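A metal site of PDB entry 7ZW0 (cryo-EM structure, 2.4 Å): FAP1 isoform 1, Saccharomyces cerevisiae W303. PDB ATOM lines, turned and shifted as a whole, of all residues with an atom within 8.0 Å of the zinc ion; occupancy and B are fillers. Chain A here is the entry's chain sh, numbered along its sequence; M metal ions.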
ATOM      1  N   MET A  69     -29.717   0.625  -1.694  1.00  0.00           N
ATOM      2  CA  MET A  69     -31.041   1.012  -1.205  1.00  0.00           C
ATOM      3  C   MET A  69     -32.008   1.607  -2.218  1.00  0.00           C
ATOM      4  O   MET A  69     -33.186   1.255  -2.219  1.00  0.00           O
ATOM      5  CB  MET A  69     -30.898   1.951  -0.006  1.00  0.00           C
ATOM      6  CG  MET A  69     -30.225   1.303   1.188  1.00  0.00           C
ATOM      7  SD  MET A  69     -30.209   2.340   2.667  1.00  0.00           S
ATOM      8  CE  MET A  69     -31.962   2.498   2.987  1.00  0.00           C
ATOM      9  N   PHE A  82     -21.348   4.096  -2.761  1.00  0.00           N
ATOM     10  CA  PHE A  82     -21.267   5.422  -2.130  1.00  0.00           C
ATOM     11  C   PHE A  82     -21.403   5.306  -0.609  1.00  0.00           C
ATOM     12  O   PHE A  82     -22.277   4.581  -0.129  1.00  0.00           O
ATOM     13  CB  PHE A  82     -22.349   6.338  -2.658  1.00  0.00           C
ATOM     14  CG  PHE A  82     -22.367   7.691  -1.998  1.00  0.00           C
ATOM     15  CD1 PHE A  82     -21.430   8.645  -2.342  1.00  0.00           C
ATOM     16  CD2 PHE A  82     -23.320   8.003  -1.052  1.00  0.00           C
ATOM     17  CE1 PHE A  82     -21.433   9.894  -1.739  1.00  0.00           C
ATOM     18  CE2 PHE A  82     -23.331   9.236  -0.436  1.00  0.00           C
ATOM     19  CZ  PHE A  82     -22.394  10.184  -0.788  1.00  0.00           C
ATOM     20  N   ALA A  83     -20.552   5.989   0.138  1.00  0.00           N
ATOM     21  CA  ALA A  83     -20.581   5.877   1.591  1.00  0.00           C
ATOM     22  C   ALA A  83     -20.918   7.188   2.267  1.00  0.00           C
ATOM     23  O   ALA A  83     -20.411   8.242   1.885  1.00  0.00           O
ATOM     24  CB  ALA A  83     -19.268   5.328   2.105  1.00  0.00           C
ATOM     25  N   CYS A  84     -21.763   7.134   3.283  1.00  0.00           N
ATOM     26  CA  CYS A  84     -22.095   8.334   4.038  1.00  0.00           C
ATOM     27  C   CYS A  84     -21.622   8.134   5.456  1.00  0.00           C
ATOM     28  O   CYS A  84     -21.879   7.092   6.040  1.00  0.00           O
ATOM     29  CB  CYS A  84     -23.599   8.610   4.019  1.00  0.00           C
ATOM     30  SG  CYS A  84     -24.123   9.937   5.119  1.00  0.00           S
ATOM     31  N   LYS A  85     -20.934   9.112   6.021  1.00  0.00           N
ATOM     32  CA  LYS A  85     -20.380   8.939   7.353  1.00  0.00           C
ATOM     33  C   LYS A  85     -21.461   8.739   8.396  1.00  0.00           C
ATOM     34  O   LYS A  85     -21.313   7.931   9.299  1.00  0.00           O
ATOM     35  CB  LYS A  85     -19.501  10.145   7.734  1.00  0.00           C
ATOM     36  CG  LYS A  85     -18.107  10.147   7.107  1.00  0.00           C
ATOM     37  CD  LYS A  85     -18.110  10.671   5.676  1.00  0.00           C
ATOM     38  CE  LYS A  85     -17.870   9.563   4.675  1.00  0.00           C
ATOM     39  NZ  LYS A  85     -18.193   9.996   3.288  1.00  0.00           N
ATOM     40  N   ARG A  86     -22.562   9.466   8.270  1.00  0.00           N
ATOM     41  CA  ARG A  86     -23.612   9.378   9.272  1.00  0.00           C
ATOM     42  C   ARG A  86     -24.235   7.978   9.354  1.00  0.00           C
ATOM     43  O   ARG A  86     -24.450   7.460  10.453  1.00  0.00           O
ATOM     44  CB  ARG A  86     -24.686  10.442   9.012  1.00  0.00           C
ATOM     45  CG  ARG A  86     -25.582  10.715  10.211  1.00  0.00           C
ATOM     46  CD  ARG A  86     -24.784  11.267  11.376  1.00  0.00           C
ATOM     47  NE  ARG A  86     -25.502  11.150  12.642  1.00  0.00           N
ATOM     48  CZ  ARG A  86     -25.383  10.122  13.479  1.00  0.00           C
ATOM     49  NH1 ARG A  86     -24.564   9.125  13.188  1.00  0.00           N
ATOM     50  NH2 ARG A  86     -26.082  10.092  14.607  1.00  0.00           N
ATOM     51  N   CYS A  87     -24.503   7.363   8.210  1.00  0.00           N
ATOM     52  CA  CYS A  87     -25.096   6.027   8.215  1.00  0.00           C
ATOM     53  C   CYS A  87     -24.110   4.900   7.994  1.00  0.00           C
ATOM     54  O   CYS A  87     -24.465   3.737   8.196  1.00  0.00           O
ATOM     55  CB  CYS A  87     -26.167   5.929   7.136  1.00  0.00           C
ATOM     56  SG  CYS A  87     -25.504   5.918   5.457  1.00  0.00           S
ATOM     57  N   TYR A  88     -22.882   5.218   7.623  1.00  0.00           N
ATOM     58  CA  TYR A  88     -21.900   4.186   7.285  1.00  0.00           C
ATOM     59  C   TYR A  88     -22.515   3.013   6.531  1.00  0.00           C
ATOM     60  O   TYR A  88     -22.265   1.848   6.861  1.00  0.00           O
ATOM     61  CB  TYR A  88     -21.106   3.736   8.512  1.00  0.00           C
ATOM     62  CG  TYR A  88     -19.973   4.679   8.828  1.00  0.00           C
ATOM     63  CD1 TYR A  88     -19.076   5.053   7.834  1.00  0.00           C
ATOM     64  CD2 TYR A  88     -19.794   5.183  10.101  1.00  0.00           C
ATOM     65  CE1 TYR A  88     -18.035   5.919   8.109  1.00  0.00           C
ATOM     66  CE2 TYR A  88     -18.760   6.050  10.388  1.00  0.00           C
ATOM     67  CZ  TYR A  88     -17.884   6.423   9.381  1.00  0.00           C
ATOM     68  OH  TYR A  88     -16.850   7.284   9.660  1.00  0.00           O
ATOM     69  N   ARG A  89     -23.308   3.310   5.507  1.00  0.00           N
ATOM     70  CA  ARG A  89     -23.942   2.279   4.714  1.00  0.00           C
ATOM     71  C   ARG A  89     -23.608   2.549   3.252  1.00  0.00           C
ATOM     72  O   ARG A  89     -23.306   3.688   2.887  1.00  0.00           O
ATOM     73  CB  ARG A  89     -25.455   2.303   4.967  1.00  0.00           C
ATOM     74  CG  ARG A  89     -26.347   1.695   3.899  1.00  0.00           C
ATOM     75  CD  ARG A  89     -26.857   0.323   4.297  1.00  0.00           C
ATOM     76  NE  ARG A  89     -27.601  -0.311   3.213  1.00  0.00           N
ATOM     77  CZ  ARG A  89     -28.229  -1.484   3.315  1.00  0.00           C
ATOM     78  NH1 ARG A  89     -28.213  -2.139   4.466  1.00  0.00           N
ATOM     79  NH2 ARG A  89     -28.867  -1.989   2.269  1.00  0.00           N
ATOM     80  N   VAL A  90     -23.646   1.531   2.406  1.00  0.00           N
ATOM     81  CA  VAL A  90     -23.285   1.700   1.001  1.00  0.00           C
ATOM     82  C   VAL A  90     -24.403   1.429   0.000  1.00  0.00           C
ATOM     83  O   VAL A  90     -25.172   0.471   0.156  1.00  0.00           O
ATOM     84  CB  VAL A  90     -22.026   0.891   0.665  1.00  0.00           C
ATOM     85  CG1 VAL A  90     -21.988   0.459  -0.780  1.00  0.00           C
ATOM     86  CG2 VAL A  90     -20.796   1.697   1.018  1.00  0.00           C
ATOM     87  N   PHE A  91     -24.541   2.294  -1.002  1.00  0.00           N
ATOM     88  CA  PHE A  91     -25.557   2.107  -2.031  1.00  0.00           C
ATOM     89  C   PHE A  91     -24.825   2.197  -3.351  1.00  0.00           C
ATOM     90  O   PHE A  91     -23.667   2.587  -3.382  1.00  0.00           O
ATOM     91  CB  PHE A  91     -26.603   3.218  -1.954  1.00  0.00           C
ATOM     92  CG  PHE A  91     -26.577   3.991  -0.672  1.00  0.00           C
ATOM     93  CD1 PHE A  91     -25.736   5.092  -0.530  1.00  0.00           C
ATOM     94  CD2 PHE A  91     -27.384   3.627   0.393  1.00  0.00           C
ATOM     95  CE1 PHE A  91     -25.708   5.806   0.658  1.00  0.00           C
ATOM     96  CE2 PHE A  91     -27.363   4.340   1.568  1.00  0.00           C
ATOM     97  CZ  PHE A  91     -26.515   5.430   1.707  1.00  0.00           C
ATOM     98  N   ILE A  96     -27.704   6.245  -5.937  1.00  0.00           N
ATOM     99  CA  ILE A  96     -27.839   7.255  -4.906  1.00  0.00           C
ATOM    100  C   ILE A  96     -27.770   8.669  -5.501  1.00  0.00           C
ATOM    101  O   ILE A  96     -28.383   9.590  -4.962  1.00  0.00           O
ATOM    102  CB  ILE A  96     -26.807   7.062  -3.770  1.00  0.00           C
ATOM    103  CG1 ILE A  96     -27.285   7.737  -2.480  1.00  0.00           C
ATOM    104  CG2 ILE A  96     -25.435   7.610  -4.147  1.00  0.00           C
ATOM    105  CD1 ILE A  96     -28.583   7.177  -1.949  1.00  0.00           C
ATOM    106  N   TRP A 112     -29.507  17.300  -0.893  1.00  0.00           N
ATOM    107  CA  TRP A 112     -29.671  15.858  -1.067  1.00  0.00           C
ATOM    108  C   TRP A 112     -29.816  15.126   0.274  1.00  0.00           C
ATOM    109  O   TRP A 112     -29.249  15.553   1.267  1.00  0.00           O
ATOM    110  CB  TRP A 112     -28.504  15.293  -1.878  1.00  0.00           C
ATOM    111  CG  TRP A 112     -27.461  14.595  -1.077  1.00  0.00           C
ATOM    112  CD1 TRP A 112     -26.418  15.160  -0.411  1.00  0.00           C
ATOM    113  CD2 TRP A 112     -27.352  13.174  -0.862  1.00  0.00           C
ATOM    114  NE1 TRP A 112     -25.671  14.184   0.200  1.00  0.00           N
ATOM    115  CE2 TRP A 112     -26.227  12.961  -0.058  1.00  0.00           C
ATOM    116  CE3 TRP A 112     -28.109  12.074  -1.276  1.00  0.00           C
ATOM    117  CZ2 TRP A 112     -25.831  11.695   0.345  1.00  0.00           C
ATOM    118  CZ3 TRP A 112     -27.713  10.826  -0.874  1.00  0.00           C
ATOM    119  CH2 TRP A 112     -26.588  10.630  -0.072  1.00  0.00           C
ATOM    120  N   LYS A 113     -30.563  14.019   0.307  1.00  0.00           N
ATOM    121  CA  LYS A 113     -30.798  13.324   1.590  1.00  0.00           C
ATOM    122  C   LYS A 113     -30.308  11.883   1.582  1.00  0.00           C
ATOM    123  O   LYS A 113     -30.504  11.175   0.607  1.00  0.00           O
ATOM    124  CB  LYS A 113     -32.291  13.361   1.937  1.00  0.00           C
ATOM    125  CG  LYS A 113     -32.605  12.897   3.353  1.00  0.00           C
ATOM    126  CD  LYS A 113     -33.969  13.390   3.792  1.00  0.00           C
ATOM    127  CE  LYS A 113     -34.120  13.261   5.297  1.00  0.00           C
ATOM    128  NZ  LYS A 113     -35.385  13.895   5.777  1.00  0.00           N
ATOM    129  N   CYS A 114     -29.687  11.453   2.661  1.00  0.00           N
ATOM    130  CA  CYS A 114     -29.242  10.077   2.754  1.00  0.00           C
ATOM    131  C   CYS A 114     -30.286   9.256   3.479  1.00  0.00           C
ATOM    132  O   CYS A 114     -30.587   9.531   4.635  1.00  0.00           O
ATOM    133  CB  CYS A 114     -27.910   9.989   3.483  1.00  0.00           C
ATOM    134  SG  CYS A 114     -27.262   8.311   3.583  1.00  0.00           S
ATOM    135  N   PRO A 115     -30.838   8.229   2.826  1.00  0.00           N
ATOM    136  CA  PRO A 115     -31.935   7.446   3.416  1.00  0.00           C
ATOM    137  C   PRO A 115     -31.640   6.633   4.675  1.00  0.00           C
ATOM    138  O   PRO A 115     -32.482   6.628   5.573  1.00  0.00           O
ATOM    139  CB  PRO A 115     -32.320   6.469   2.297  1.00  0.00           C
ATOM    140  CG  PRO A 115     -31.726   7.041   1.043  1.00  0.00           C
ATOM    141  CD  PRO A 115     -30.485   7.749   1.478  1.00  0.00           C
ATOM    142  N   ASN A 116     -30.502   5.966   4.752  1.00  0.00           N
ATOM    143  CA  ASN A 116     -30.255   5.094   5.904  1.00  0.00           C
ATOM    144  C   ASN A 116     -30.201   5.851   7.212  1.00  0.00           C
ATOM    145  O   ASN A 116     -30.760   5.406   8.219  1.00  0.00           O
ATOM    146  CB  ASN A 116     -28.977   4.278   5.704  1.00  0.00           C
ATOM    147  CG  ASN A 116     -28.932   3.048   6.604  1.00  0.00           C
ATOM    148  OD1 ASN A 116     -29.866   2.242   6.605  1.00  0.00           O
ATOM    149  ND2 ASN A 116     -27.848   2.894   7.345  1.00  0.00           N
ATOM    150  N   CYS A 117     -29.547   7.003   7.219  1.00  0.00           N
ATOM    151  CA  CYS A 117     -29.512   7.827   8.419  1.00  0.00           C
ATOM    152  C   CYS A 117     -30.619   8.849   8.374  1.00  0.00           C
ATOM    153  O   CYS A 117     -30.747   9.655   9.302  1.00  0.00           O
ATOM    154  CB  CYS A 117     -28.165   8.523   8.554  1.00  0.00           C
ATOM    155  SG  CYS A 117     -27.556   9.212   7.010  1.00  0.00           S
ATOM    156  N   TYR A 118     -31.407   8.842   7.304  1.00  0.00           N
ATOM    157  CA  TYR A 118     -32.469   9.830   7.132  1.00  0.00           C
ATOM    158  C   TYR A 118     -31.862  11.188   7.409  1.00  0.00           C
ATOM    159  O   TYR A 118     -32.438  12.000   8.129  1.00  0.00           O
ATOM    160  CB  TYR A 118     -33.654   9.537   8.068  1.00  0.00           C
ATOM    161  CG  TYR A 118     -34.960  10.112   7.597  1.00  0.00           C
ATOM    162  CD1 TYR A 118     -35.507   9.749   6.371  1.00  0.00           C
ATOM    163  CD2 TYR A 118     -35.664  11.018   8.381  1.00  0.00           C
ATOM    164  CE1 TYR A 118     -36.702  10.280   5.939  1.00  0.00           C
ATOM    165  CE2 TYR A 118     -36.866  11.550   7.961  1.00  0.00           C
ATOM    166  CZ  TYR A 118     -37.385  11.169   6.737  1.00  0.00           C
ATOM    167  OH  TYR A 118     -38.586  11.694   6.309  1.00  0.00           O
ATOM    168  N   TYR A 119     -30.686  11.440   6.844  1.00  0.00           N
ATOM    169  CA  TYR A 119     -29.988  12.691   7.119  1.00  0.00           C
ATOM    170  C   TYR A 119     -29.725  13.457   5.856  1.00  0.00           C
ATOM    171  O   TYR A 119     -29.176  12.917   4.897  1.00  0.00           O
ATOM    172  CB  TYR A 119     -28.701  12.394   7.904  1.00  0.00           C
ATOM    173  CG  TYR A 119     -27.447  13.143   7.488  1.00  0.00           C
ATOM    174  CD1 TYR A 119     -26.593  12.633   6.523  1.00  0.00           C
ATOM    175  CD2 TYR A 119     -27.090  14.332   8.108  1.00  0.00           C
ATOM    176  CE1 TYR A 119     -25.447  13.299   6.147  1.00  0.00           C
ATOM    177  CE2 TYR A 119     -25.943  15.004   7.740  1.00  0.00           C
ATOM    178  CZ  TYR A 119     -25.132  14.488   6.766  1.00  0.00           C
ATOM    179  OH  TYR A 119     -23.986  15.154   6.391  1.00  0.00           O
ATOM    180  N   VAL A 120     -30.144  14.716   5.821  1.00  0.00           N
ATOM    181  CA  VAL A 120     -29.882  15.540   4.652  1.00  0.00           C
ATOM    182  C   VAL A 120     -28.456  16.040   4.652  1.00  0.00           C
ATOM    183  O   VAL A 120     -27.898  16.338   5.699  1.00  0.00           O
ATOM    184  CB  VAL A 120     -30.832  16.746   4.613  1.00  0.00           C
ATOM    185  CG1 VAL A 120     -31.650  16.734   3.325  1.00  0.00           C
ATOM    186  CG2 VAL A 120     -31.745  16.730   5.817  1.00  0.00           C
ATOM    187  N   SER A 121     -27.861  16.154   3.478  1.00  0.00           N
ATOM    188  CA  SER A 121     -26.509  16.699   3.362  1.00  0.00           C
ATOM    189  C   SER A 121     -26.544  17.747   2.275  1.00  0.00           C
ATOM    190  O   SER A 121     -27.515  17.805   1.511  1.00  0.00           O
ATOM    191  CB  SER A 121     -25.480  15.602   3.091  1.00  0.00           C
ATOM    192  OG  SER A 121     -24.159  16.125   3.083  1.00  0.00           O
HETATM  193 ZN    ZN M   1     -25.986   8.236   5.183  1.00  0.00          ZN
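The side-chain sulfur (SG) of Cys 84 lies close to the backbone NH (N) of Arg 86, at 3.5 Å. The side-chain sulfur (SG) of Cys 87 sits close to the backbone NH (N) of Arg 89. N of Cys 114 sits at hydrogen-bond distance from O of Tyr 119, at 2.7 Å.
The zinc ion is bound by SG of Cys 114 (2.0 Å), SG of Cys 87 (2.4 Å), SG of Cys 84 (2.5 Å) and SG of Cys 117 (2.6 Å).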
